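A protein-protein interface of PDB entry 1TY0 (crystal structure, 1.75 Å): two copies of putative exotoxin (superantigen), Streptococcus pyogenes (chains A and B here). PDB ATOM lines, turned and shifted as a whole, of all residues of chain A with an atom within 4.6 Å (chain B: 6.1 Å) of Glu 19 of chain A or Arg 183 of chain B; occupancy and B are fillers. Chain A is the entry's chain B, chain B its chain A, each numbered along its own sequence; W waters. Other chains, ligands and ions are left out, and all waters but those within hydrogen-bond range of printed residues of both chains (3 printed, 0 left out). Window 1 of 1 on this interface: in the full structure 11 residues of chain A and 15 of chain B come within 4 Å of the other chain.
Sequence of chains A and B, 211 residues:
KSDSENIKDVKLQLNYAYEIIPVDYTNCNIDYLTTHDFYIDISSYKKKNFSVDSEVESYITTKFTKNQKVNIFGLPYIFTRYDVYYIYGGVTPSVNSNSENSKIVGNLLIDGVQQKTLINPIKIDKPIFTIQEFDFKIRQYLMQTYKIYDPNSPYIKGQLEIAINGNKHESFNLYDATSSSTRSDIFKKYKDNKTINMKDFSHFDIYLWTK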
ATOM      1  N   ASN A  15     -30.882   7.600  23.090  1.00  0.00           N
ATOM      2  CA  ASN A  15     -30.336   8.700  22.308  1.00  0.00           C
ATOM      3  C   ASN A  15     -28.992   8.269  21.731  1.00  0.00           C
ATOM      4  O   ASN A  15     -28.703   8.514  20.559  1.00  0.00           O
ATOM      5  CB  ASN A  15     -30.177   9.933  23.206  1.00  0.00           C
ATOM      6  CG  ASN A  15     -30.472  11.232  22.477  1.00  0.00           C
ATOM      7  OD1 ASN A  15     -31.207  11.251  21.490  1.00  0.00           O
ATOM      8  ND2 ASN A  15     -29.915  12.330  22.976  1.00  0.00           N
ATOM      9  N   TYR A  16     -28.182   7.606  22.552  1.00  0.00           N
ATOM     10  CA  TYR A  16     -26.875   7.129  22.109  1.00  0.00           C
ATOM     11  C   TYR A  16     -27.059   6.089  21.015  1.00  0.00           C
ATOM     12  O   TYR A  16     -26.490   6.189  19.932  1.00  0.00           O
ATOM     13  CB  TYR A  16     -26.102   6.457  23.253  1.00  0.00           C
ATOM     14  CG  TYR A  16     -25.771   7.313  24.455  1.00  0.00           C
ATOM     15  CD1 TYR A  16     -25.302   8.617  24.310  1.00  0.00           C
ATOM     16  CD2 TYR A  16     -25.858   6.784  25.745  1.00  0.00           C
ATOM     17  CE1 TYR A  16     -24.922   9.375  25.420  1.00  0.00           C
ATOM     18  CE2 TYR A  16     -25.483   7.531  26.860  1.00  0.00           C
ATOM     19  CZ  TYR A  16     -25.015   8.823  26.692  1.00  0.00           C
ATOM     20  OH  TYR A  16     -24.633   9.556  27.791  1.00  0.00           O
ATOM     21  N   ALA A  17     -27.871   5.083  21.318  1.00  0.00           N
ATOM     22  CA  ALA A  17     -28.123   3.986  20.399  1.00  0.00           C
ATOM     23  C   ALA A  17     -28.612   4.345  18.995  1.00  0.00           C
ATOM     24  O   ALA A  17     -28.088   3.834  18.006  1.00  0.00           O
ATOM     25  CB  ALA A  17     -29.097   2.998  21.046  1.00  0.00           C
ATOM     26  N   TYR A  18     -29.607   5.223  18.902  1.00  0.00           N
ATOM     27  CA  TYR A  18     -30.178   5.574  17.611  1.00  0.00           C
ATOM     28  C   TYR A  18     -29.524   6.696  16.803  1.00  0.00           C
ATOM     29  O   TYR A  18     -29.862   6.897  15.635  1.00  0.00           O
ATOM     30  CB  TYR A  18     -31.679   5.831  17.795  1.00  0.00           C
ATOM     31  CG  TYR A  18     -32.465   4.543  17.930  1.00  0.00           C
ATOM     32  CD1 TYR A  18     -32.763   3.771  16.805  1.00  0.00           C
ATOM     33  CD2 TYR A  18     -32.878   4.075  19.181  1.00  0.00           C
ATOM     34  CE1 TYR A  18     -33.453   2.561  16.917  1.00  0.00           C
ATOM     35  CE2 TYR A  18     -33.567   2.858  19.305  1.00  0.00           C
ATOM     36  CZ  TYR A  18     -33.849   2.111  18.168  1.00  0.00           C
ATOM     37  OH  TYR A  18     -34.526   0.911  18.268  1.00  0.00           O
ATOM     38  N   GLU A  19     -28.582   7.412  17.408  1.00  0.00           N
ATOM     39  CA  GLU A  19     -27.883   8.490  16.702  1.00  0.00           C
ATOM     40  C   GLU A  19     -26.737   7.842  15.929  1.00  0.00           C
ATOM     41  O   GLU A  19     -25.570   7.950  16.317  1.00  0.00           O
ATOM     42  CB  GLU A  19     -27.319   9.507  17.701  1.00  0.00           C
ATOM     43  CG  GLU A  19     -26.680  10.727  17.034  1.00  0.00           C
ATOM     44  CD  GLU A  19     -27.712  11.715  16.525  1.00  0.00           C
ATOM     45  OE1 GLU A  19     -28.856  11.295  16.246  1.00  0.00           O
ATOM     46  OE2 GLU A  19     -27.376  12.912  16.391  1.00  0.00           O
ATOM     47  N   ILE A  20     -27.065   7.177  14.828  1.00  0.00           N
ATOM     48  CA  ILE A  20     -26.040   6.485  14.060  1.00  0.00           C
ATOM     49  C   ILE A  20     -26.369   6.380  12.578  1.00  0.00           C
ATOM     50  O   ILE A  20     -27.524   6.514  12.171  1.00  0.00           O
ATOM     51  CB  ILE A  20     -25.838   5.060  14.638  1.00  0.00           C
ATOM     52  CG1 ILE A  20     -24.587   4.409  14.045  1.00  0.00           C
ATOM     53  CG2 ILE A  20     -27.069   4.207  14.342  1.00  0.00           C
ATOM     54  CD1 ILE A  20     -24.166   3.158  14.773  1.00  0.00           C
ATOM     55  N   GLN A 140     -35.530   8.708  14.202  1.00  0.00           N
ATOM     56  CA  GLN A 140     -34.664   9.824  13.837  1.00  0.00           C
ATOM     57  C   GLN A 140     -35.513  11.074  13.578  1.00  0.00           C
ATOM     58  O   GLN A 140     -35.139  12.185  13.972  1.00  0.00           O
ATOM     59  CB  GLN A 140     -33.820   9.468  12.609  1.00  0.00           C
ATOM     60  CG  GLN A 140     -32.442   8.919  12.975  1.00  0.00           C
ATOM     61  CD  GLN A 140     -31.585   9.954  13.687  1.00  0.00           C
ATOM     62  OE1 GLN A 140     -31.669  11.145  13.393  1.00  0.00           O
ATOM     63  NE2 GLN A 140     -30.744   9.503  14.617  1.00  0.00           N
ATOM     64  N   MET A 143     -36.420  12.268  16.955  1.00  0.00           N
ATOM     65  CA  MET A 143     -35.268  12.789  17.677  1.00  0.00           C
ATOM     66  C   MET A 143     -34.913  14.168  17.126  1.00  0.00           C
ATOM     67  O   MET A 143     -34.646  15.104  17.881  1.00  0.00           O
ATOM     68  CB  MET A 143     -34.087  11.832  17.519  1.00  0.00           C
ATOM     69  CG  MET A 143     -34.253  10.552  18.315  1.00  0.00           C
ATOM     70  SD  MET A 143     -33.183   9.242  17.707  1.00  0.00           S
ATOM     71  CE  MET A 143     -31.607   9.801  18.293  1.00  0.00           C
ATOM     72  N   ARG A 183     -26.394  -0.926  22.973  1.00  0.00           N
ATOM     73  CA  ARG A 183     -27.003  -0.898  21.654  1.00  0.00           C
ATOM     74  C   ARG A 183     -27.476  -2.300  21.306  1.00  0.00           C
ATOM     75  O   ARG A 183     -28.538  -2.474  20.711  1.00  0.00           O
ATOM     76  CB  ARG A 183     -26.007  -0.409  20.606  1.00  0.00           C
ATOM     77  CG  ARG A 183     -25.916   1.100  20.540  1.00  0.00           C
ATOM     78  CD  ARG A 183     -24.954   1.548  19.458  1.00  0.00           C
ATOM     79  NE  ARG A 183     -25.136   2.958  19.131  1.00  0.00           N
ATOM     80  CZ  ARG A 183     -24.231   3.702  18.503  1.00  0.00           C
ATOM     81  NH1 ARG A 183     -23.074   3.172  18.138  1.00  0.00           N
ATOM     82  NH2 ARG A 183     -24.486   4.976  18.237  1.00  0.00           N
ATOM     83  N   ASN B  15     -16.470   7.982  24.645  1.00  0.00           N
ATOM     84  CA  ASN B  15     -16.795   6.651  24.160  1.00  0.00           C
ATOM     85  C   ASN B  15     -18.022   6.737  23.267  1.00  0.00           C
ATOM     86  O   ASN B  15     -18.062   6.139  22.191  1.00  0.00           O
ATOM     87  CB  ASN B  15     -17.042   5.699  25.331  1.00  0.00           C
ATOM     88  CG  ASN B  15     -17.000   4.249  24.905  1.00  0.00           C
ATOM     89  OD1 ASN B  15     -18.022   3.666  24.544  1.00  0.00           O
ATOM     90  ND2 ASN B  15     -15.807   3.665  24.917  1.00  0.00           N
ATOM     91  N   TYR B  16     -19.017   7.500  23.703  1.00  0.00           N
ATOM     92  CA  TYR B  16     -20.222   7.663  22.906  1.00  0.00           C
ATOM     93  C   TYR B  16     -19.951   8.411  21.603  1.00  0.00           C
ATOM     94  O   TYR B  16     -20.402   7.997  20.538  1.00  0.00           O
ATOM     95  CB  TYR B  16     -21.294   8.430  23.677  1.00  0.00           C
ATOM     96  CG  TYR B  16     -22.309   9.063  22.751  1.00  0.00           C
ATOM     97  CD1 TYR B  16     -23.119   8.276  21.930  1.00  0.00           C
ATOM     98  CD2 TYR B  16     -22.422  10.449  22.653  1.00  0.00           C
ATOM     99  CE1 TYR B  16     -24.015   8.857  21.035  1.00  0.00           C
ATOM    100  CE2 TYR B  16     -23.313  11.038  21.760  1.00  0.00           C
ATOM    101  CZ  TYR B  16     -24.105  10.237  20.955  1.00  0.00           C
ATOM    102  OH  TYR B  16     -24.984  10.815  20.069  1.00  0.00           O
ATOM    103  N   ALA B  17     -19.230   9.523  21.699  1.00  0.00           N
ATOM    104  CA  ALA B  17     -18.933  10.339  20.528  1.00  0.00           C
ATOM    105  C   ALA B  17     -18.235   9.572  19.412  1.00  0.00           C
ATOM    106  O   ALA B  17     -18.614   9.689  18.247  1.00  0.00           O
ATOM    107  CB  ALA B  17     -18.087  11.550  20.933  1.00  0.00           C
ATOM    108  N   TYR B  18     -17.229   8.777  19.765  1.00  0.00           N
ATOM    109  CA  TYR B  18     -16.476   8.034  18.763  1.00  0.00           C
ATOM    110  C   TYR B  18     -17.003   6.650  18.362  1.00  0.00           C
ATOM    111  O   TYR B  18     -16.438   6.006  17.484  1.00  0.00           O
ATOM    112  CB  TYR B  18     -15.005   7.966  19.194  1.00  0.00           C
ATOM    113  CG  TYR B  18     -14.273   9.278  18.965  1.00  0.00           C
ATOM    114  CD1 TYR B  18     -13.766   9.602  17.710  1.00  0.00           C
ATOM    115  CD2 TYR B  18     -14.123  10.210  19.996  1.00  0.00           C
ATOM    116  CE1 TYR B  18     -13.123  10.824  17.476  1.00  0.00           C
ATOM    117  CE2 TYR B  18     -13.482  11.440  19.773  1.00  0.00           C
ATOM    118  CZ  TYR B  18     -12.986  11.736  18.509  1.00  0.00           C
ATOM    119  OH  TYR B  18     -12.348  12.938  18.279  1.00  0.00           O
ATOM    120  N   GLU B  19     -18.070   6.184  19.008  1.00  0.00           N
ATOM    121  CA  GLU B  19     -18.678   4.899  18.638  1.00  0.00           C
ATOM    122  C   GLU B  19     -19.659   5.302  17.546  1.00  0.00           C
ATOM    123  O   GLU B  19     -20.860   5.395  17.774  1.00  0.00           O
ATOM    124  CB  GLU B  19     -19.430   4.291  19.824  1.00  0.00           C
ATOM    125  CG  GLU B  19     -18.549   3.482  20.766  1.00  0.00           C
ATOM    126  CD  GLU B  19     -18.158   2.142  20.178  1.00  0.00           C
ATOM    127  OE1 GLU B  19     -19.062   1.308  19.941  1.00  0.00           O
ATOM    128  OE2 GLU B  19     -16.951   1.919  19.947  1.00  0.00           O
ATOM    129  N   ILE B  20     -19.126   5.539  16.354  1.00  0.00           N
ATOM    130  CA  ILE B  20     -19.930   6.017  15.243  1.00  0.00           C
ATOM    131  C   ILE B  20     -19.411   5.536  13.889  1.00  0.00           C
ATOM    132  O   ILE B  20     -18.265   5.110  13.765  1.00  0.00           O
ATOM    133  CB  ILE B  20     -19.924   7.560  15.269  1.00  0.00           C
ATOM    134  CG1 ILE B  20     -20.759   8.141  14.131  1.00  0.00           C
ATOM    135  CG2 ILE B  20     -18.494   8.057  15.177  1.00  0.00           C
ATOM    136  CD1 ILE B  20     -20.839   9.651  14.184  1.00  0.00           C
ATOM    137  N   PRO B  76     -19.967  12.532  11.283  1.00  0.00           N
ATOM    138  CA  PRO B  76     -21.179  13.360  11.332  1.00  0.00           C
ATOM    139  C   PRO B  76     -21.463  13.840  12.750  1.00  0.00           C
ATOM    140  O   PRO B  76     -21.361  13.063  13.697  1.00  0.00           O
ATOM    141  CB  PRO B  76     -22.258  12.415  10.810  1.00  0.00           C
ATOM    142  CG  PRO B  76     -21.806  11.083  11.352  1.00  0.00           C
ATOM    143  CD  PRO B  76     -20.307  11.113  11.054  1.00  0.00           C
ATOM    144  N   TYR B  77     -21.820  15.114  12.899  1.00  0.00           N
ATOM    145  CA  TYR B  77     -22.092  15.652  14.229  1.00  0.00           C
ATOM    146  C   TYR B  77     -23.570  15.952  14.473  1.00  0.00           C
ATOM    147  O   TYR B  77     -23.988  16.218  15.606  1.00  0.00           O
ATOM    148  CB  TYR B  77     -21.239  16.907  14.472  1.00  0.00           C
ATOM    149  CG  TYR B  77     -21.483  18.048  13.507  1.00  0.00           C
ATOM    150  CD1 TYR B  77     -22.523  18.956  13.715  1.00  0.00           C
ATOM    151  CD2 TYR B  77     -20.670  18.225  12.391  1.00  0.00           C
ATOM    152  CE1 TYR B  77     -22.743  20.015  12.832  1.00  0.00           C
ATOM    153  CE2 TYR B  77     -20.883  19.278  11.499  1.00  0.00           C
ATOM    154  CZ  TYR B  77     -21.919  20.168  11.724  1.00  0.00           C
ATOM    155  OH  TYR B  77     -22.134  21.207  10.843  1.00  0.00           O
ATOM    156  N   ILE B  78     -24.362  15.903  13.413  1.00  0.00           N
ATOM    157  CA  ILE B  78     -25.790  16.157  13.529  1.00  0.00           C
ATOM    158  C   ILE B  78     -26.498  15.591  12.310  1.00  0.00           C
ATOM    159  O   ILE B  78     -25.903  15.493  11.238  1.00  0.00           O
ATOM    160  CB  ILE B  78     -26.083  17.674  13.625  1.00  0.00           C
ATOM    161  CG1 ILE B  78     -27.527  17.903  14.066  1.00  0.00           C
ATOM    162  CG2 ILE B  78     -25.848  18.351  12.282  1.00  0.00           C
ATOM    163  CD1 ILE B  78     -27.788  17.536  15.509  1.00  0.00           C
ATOM    164  N   PHE B  79     -27.757  15.201  12.489  1.00  0.00           N
ATOM    165  CA  PHE B  79     -28.570  14.674  11.397  1.00  0.00           C
ATOM    166  C   PHE B  79     -29.799  15.560  11.247  1.00  0.00           C
ATOM    167  O   PHE B  79     -30.299  16.121  12.229  1.00  0.00           O
ATOM    168  CB  PHE B  79     -29.034  13.237  11.685  1.00  0.00           C
ATOM    169  CG  PHE B  79     -27.916  12.246  11.818  1.00  0.00           C
ATOM    170  CD1 PHE B  79     -26.984  12.083  10.799  1.00  0.00           C
ATOM    171  CD2 PHE B  79     -27.805  11.464  12.960  1.00  0.00           C
ATOM    172  CE1 PHE B  79     -25.956  11.152  10.917  1.00  0.00           C
ATOM    173  CE2 PHE B  79     -26.777  10.526  13.087  1.00  0.00           C
ATOM    174  CZ  PHE B  79     -25.854  10.373  12.062  1.00  0.00           C
ATOM    175  N   TYR B  88     -17.242  18.197   9.858  1.00  0.00           N
ATOM    176  CA  TYR B  88     -16.269  19.284   9.981  1.00  0.00           C
ATOM    177  C   TYR B  88     -15.016  18.778   9.280  1.00  0.00           C
ATOM    178  O   TYR B  88     -14.535  17.686   9.589  1.00  0.00           O
ATOM    179  CB  TYR B  88     -15.938  19.571  11.449  1.00  0.00           C
ATOM    180  CG  TYR B  88     -17.075  20.141  12.256  1.00  0.00           C
ATOM    181  CD1 TYR B  88     -17.747  21.292  11.840  1.00  0.00           C
ATOM    182  CD2 TYR B  88     -17.451  19.557  13.466  1.00  0.00           C
ATOM    183  CE1 TYR B  88     -18.764  21.852  12.615  1.00  0.00           C
ATOM    184  CE2 TYR B  88     -18.463  20.110  14.247  1.00  0.00           C
ATOM    185  CZ  TYR B  88     -19.114  21.256  13.817  1.00  0.00           C
ATOM    186  OH  TYR B  88     -20.117  21.810  14.594  1.00  0.00           O
ATOM    187  N   SER B 181     -19.877  17.627  26.804  1.00  0.00           N
ATOM    188  CA  SER B 181     -19.537  17.691  25.384  1.00  0.00           C
ATOM    189  C   SER B 181     -20.395  16.855  24.434  1.00  0.00           C
ATOM    190  O   SER B 181     -20.599  15.660  24.655  1.00  0.00           O
ATOM    191  CB  SER B 181     -18.072  17.293  25.181  1.00  0.00           C
ATOM    192  OG  SER B 181     -17.197  18.150  25.890  1.00  0.00           O
ATOM    193  N   THR B 182     -20.875  17.502  23.372  1.00  0.00           N
ATOM    194  CA  THR B 182     -21.674  16.851  22.329  1.00  0.00           C
ATOM    195  C   THR B 182     -20.696  16.451  21.228  1.00  0.00           C
ATOM    196  O   THR B 182     -19.531  16.838  21.271  1.00  0.00           O
ATOM    197  CB  THR B 182     -22.690  17.821  21.689  1.00  0.00           C
ATOM    198  OG1 THR B 182     -21.989  18.895  21.047  1.00  0.00           O
ATOM    199  CG2 THR B 182     -23.629  18.386  22.737  1.00  0.00           C
ATOM    200  N   ARG B 183     -21.158  15.695  20.235  1.00  0.00           N
ATOM    201  CA  ARG B 183     -20.269  15.308  19.147  1.00  0.00           C
ATOM    202  C   ARG B 183     -19.784  16.556  18.422  1.00  0.00           C
ATOM    203  O   ARG B 183     -18.624  16.637  18.026  1.00  0.00           O
ATOM    204  CB  ARG B 183     -20.973  14.360  18.173  1.00  0.00           C
ATOM    205  CG  ARG B 183     -20.825  12.903  18.569  1.00  0.00           C
ATOM    206  CD  ARG B 183     -21.625  11.973  17.666  1.00  0.00           C
ATOM    207  NE  ARG B 183     -21.391  10.582  18.038  1.00  0.00           N
ATOM    208  CZ  ARG B 183     -22.236   9.584  17.798  1.00  0.00           C
ATOM    209  NH1 ARG B 183     -23.388   9.813  17.179  1.00  0.00           N
ATOM    210  NH2 ARG B 183     -21.926   8.353  18.179  1.00  0.00           N
ATOM    211  N   SER B 184     -20.672  17.533  18.262  1.00  0.00           N
ATOM    212  CA  SER B 184     -20.302  18.779  17.606  1.00  0.00           C
ATOM    213  C   SER B 184     -19.144  19.431  18.357  1.00  0.00           C
ATOM    214  O   SER B 184     -18.167  19.863  17.747  1.00  0.00           O
ATOM    215  CB  SER B 184     -21.485  19.745  17.572  1.00  0.00           C
ATOM    216  OG  SER B 184     -21.117  20.964  16.954  1.00  0.00           O
ATOM    217  N   ASP B 185     -19.258  19.506  19.682  1.00  0.00           N
ATOM    218  CA  ASP B 185     -18.202  20.115  20.495  1.00  0.00           C
ATOM    219  C   ASP B 185     -16.867  19.402  20.317  1.00  0.00           C
ATOM    220  O   ASP B 185     -15.832  20.047  20.139  1.00  0.00           O
ATOM    221  CB  ASP B 185     -18.550  20.078  21.988  1.00  0.00           C
ATOM    222  CG  ASP B 185     -19.760  20.915  22.339  1.00  0.00           C
ATOM    223  OD1 ASP B 185     -19.979  21.963  21.698  1.00  0.00           O
ATOM    224  OD2 ASP B 185     -20.478  20.528  23.281  1.00  0.00           O
ATOM    225  N   ILE B 186     -16.902  18.072  20.369  1.00  0.00           N
ATOM    226  CA  ILE B 186     -15.693  17.256  20.262  1.00  0.00           C
ATOM    227  C   ILE B 186     -15.080  17.211  18.869  1.00  0.00           C
ATOM    228  O   ILE B 186     -13.858  17.153  18.722  1.00  0.00           O
ATOM    229  CB  ILE B 186     -15.975  15.808  20.743  1.00  0.00           C
ATOM    230  CG1 ILE B 186     -16.325  15.823  22.237  1.00  0.00           C
ATOM    231  CG2 ILE B 186     -14.755  14.920  20.517  1.00  0.00           C
ATOM    232  CD1 ILE B 186     -16.932  14.536  22.747  1.00  0.00           C
ATOM    233  N   PHE B 187     -15.922  17.250  17.843  1.00  0.00           N
ATOM    234  CA  PHE B 187     -15.436  17.188  16.469  1.00  0.00           C
ATOM    235  C   PHE B 187     -15.038  18.542  15.878  1.00  0.00           C
ATOM    236  O   PHE B 187     -14.394  18.591  14.836  1.00  0.00           O
ATOM    237  CB  PHE B 187     -16.491  16.549  15.551  1.00  0.00           C
ATOM    238  CG  PHE B 187     -16.875  15.140  15.921  1.00  0.00           C
ATOM    239  CD1 PHE B 187     -16.091  14.371  16.780  1.00  0.00           C
ATOM    240  CD2 PHE B 187     -18.023  14.568  15.369  1.00  0.00           C
ATOM    241  CE1 PHE B 187     -16.447  13.052  17.084  1.00  0.00           C
ATOM    242  CE2 PHE B 187     -18.387  13.255  15.663  1.00  0.00           C
ATOM    243  CZ  PHE B 187     -17.598  12.494  16.522  1.00  0.00           C
ATOM    244  N   LYS B 188     -15.413  19.638  16.531  1.00  0.00           N
ATOM    245  CA  LYS B 188     -15.090  20.959  16.004  1.00  0.00           C
ATOM    246  C   LYS B 188     -13.606  21.148  15.719  1.00  0.00           C
ATOM    247  O   LYS B 188     -13.236  21.911  14.832  1.00  0.00           O
ATOM    248  CB  LYS B 188     -15.585  22.054  16.958  1.00  0.00           C
ATOM    249  CG  LYS B 188     -16.673  22.934  16.350  1.00  0.00           C
ATOM    250  CD  LYS B 188     -17.277  23.879  17.376  1.00  0.00           C
ATOM    251  CE  LYS B 188     -18.258  24.846  16.733  1.00  0.00           C
ATOM    252  NZ  LYS B 188     -19.365  24.153  16.019  1.00  0.00           N
HETATM  253  O   HOH W   1     -28.849  14.716  15.118  1.00  0.00           O
HETATM  254  O   HOH W   2     -23.828   9.108  14.174  1.00  0.00           O
HETATM  255  O   HOH W   3     -24.945  13.706  16.744  1.00  0.00           O
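NH1 of Arg 183 of chain A sits at hydrogen-bond distance from O of Glu 19 of chain B.
The guanidinium group of Arg 183 of chain B is in hydrogen-bond range of the backbone carbonyl oxygen of Glu 19 of chain A, 3.0 Å away.
The backbone carbonyl oxygen (O) of Ala 17 of chain A sits at hydrogen-bond distance from the guanidinium group (NE) of Arg 183 of chain A.
The guanidinium group (NE) of Arg 183 of chain B is in hydrogen-bond range of the backbone carbonyl oxygen (O) of Ala 17 of chain B (2.9 Å).
The backbone carbonyl oxygen of Glu 19 of chain B is in hydrogen-bond range of the guanidinium group of Arg 183 of chain B.
OE1 of Glu 19 of chain A lies within hydrogen-bond range of NE2 of Gln 140 of chain A (3.1 Å).
O of Tyr 16 of chain A is in hydrogen-bond range of NH2 of Arg 183 of chain A (2.9 Å).
NH2 of Arg 183 of chain B lies within hydrogen-bond range of O of Tyr 16 of chain B (2.8 Å).
CD1 of Tyr 16 of chain B touches CD1 of Tyr 16 of chain A, at 3.2 Å.
Glu 19 of chain A touches Tyr 16 of chain B.
Glu 19 of chain A touches Phe 79 of chain B (OE1 to CD2, 3.5 Å).
Phe 79 of chain B touches Ile 20 of chain A (CE2 to N, 3.8 Å).
Phe 79 of chain B touches Gln 140 of chain A (CB to OE1, 3.8 Å).
Of chain B, only Tyr 16 (3.5 Å), Phe 79 (3.5 Å) and Arg 183 (3.0 Å) come within 4 Å of Glu 19 of chain A.
Of the printed residues of chain B, Arg 183 of chain A touches Glu 19 (3.2 Å).
Asn 15 of chain B touches none of the printed residues of chain A.
Of the printed residues of chain A, Phe 79 of chain B touches Glu 19 (3.5 Å), Ile 20 (3.8 Å) and Gln 140 (3.8 Å).
Of chain A, only Glu 19 (3.0 Å) comes within 4 Å of Arg 183 of chain B.
Lys 188 of chain B touches none of the printed residues of chain A.
The nearest residue of chain B that does not touch Glu 19 of chain A is Ile 78 of chain B (4.6 Å).
The nearest residue of chain A that does not touch Arg 183 of chain B is Arg 183 of chain A (4.2 Å).
The nearest printed residue of chain A that does not touch Glu 19 of chain B is Ile 20 of chain A (5.0 Å).
Hydrophobic or aromatic side chains of chain B within 4 Å of the printed part of chain A: Tyr 16 and Phe 79.
Of the 9 printed residues of chain A, 5 touch a printed residue of chain B.
Hydrophobic or aromatic side chains of chain A that line the printed part of chain B: Tyr 16.
Among the printed residues, no Asp or Glu carboxylate lies within 4 Å of a Lys or Arg side-chain nitrogen of the other chain.
Tyr 16 of chain A touches its own counterpart, Tyr 16 of chain B.
Glu 19 of chain A touches Tyr 16 of chain B, but with the chains exchanged Tyr 16 of chain A does not touch Glu 19 of chain B (6.1 Å).
Glu 19 of chain A touches Arg 183 of chain B, and with the chains exchanged Arg 183 of chain A touches Glu 19 of chain B.
7 positions are printed for both chains.
Water W3 lies within hydrogen-bond range of OE2 of Glu 19 of chain A (2.6 Å) and O of Tyr 77 of chain B (2.9 Å).
Water W1 bridges the side-chain carboxylate (OE2) of Glu 19 of chain A and the backbone NH (N) of Phe 79 of chain B.
Water W2 bridges O of Glu 19 of chain A (3.0 Å) and NH1 of Arg 183 of chain B (3.1 Å).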
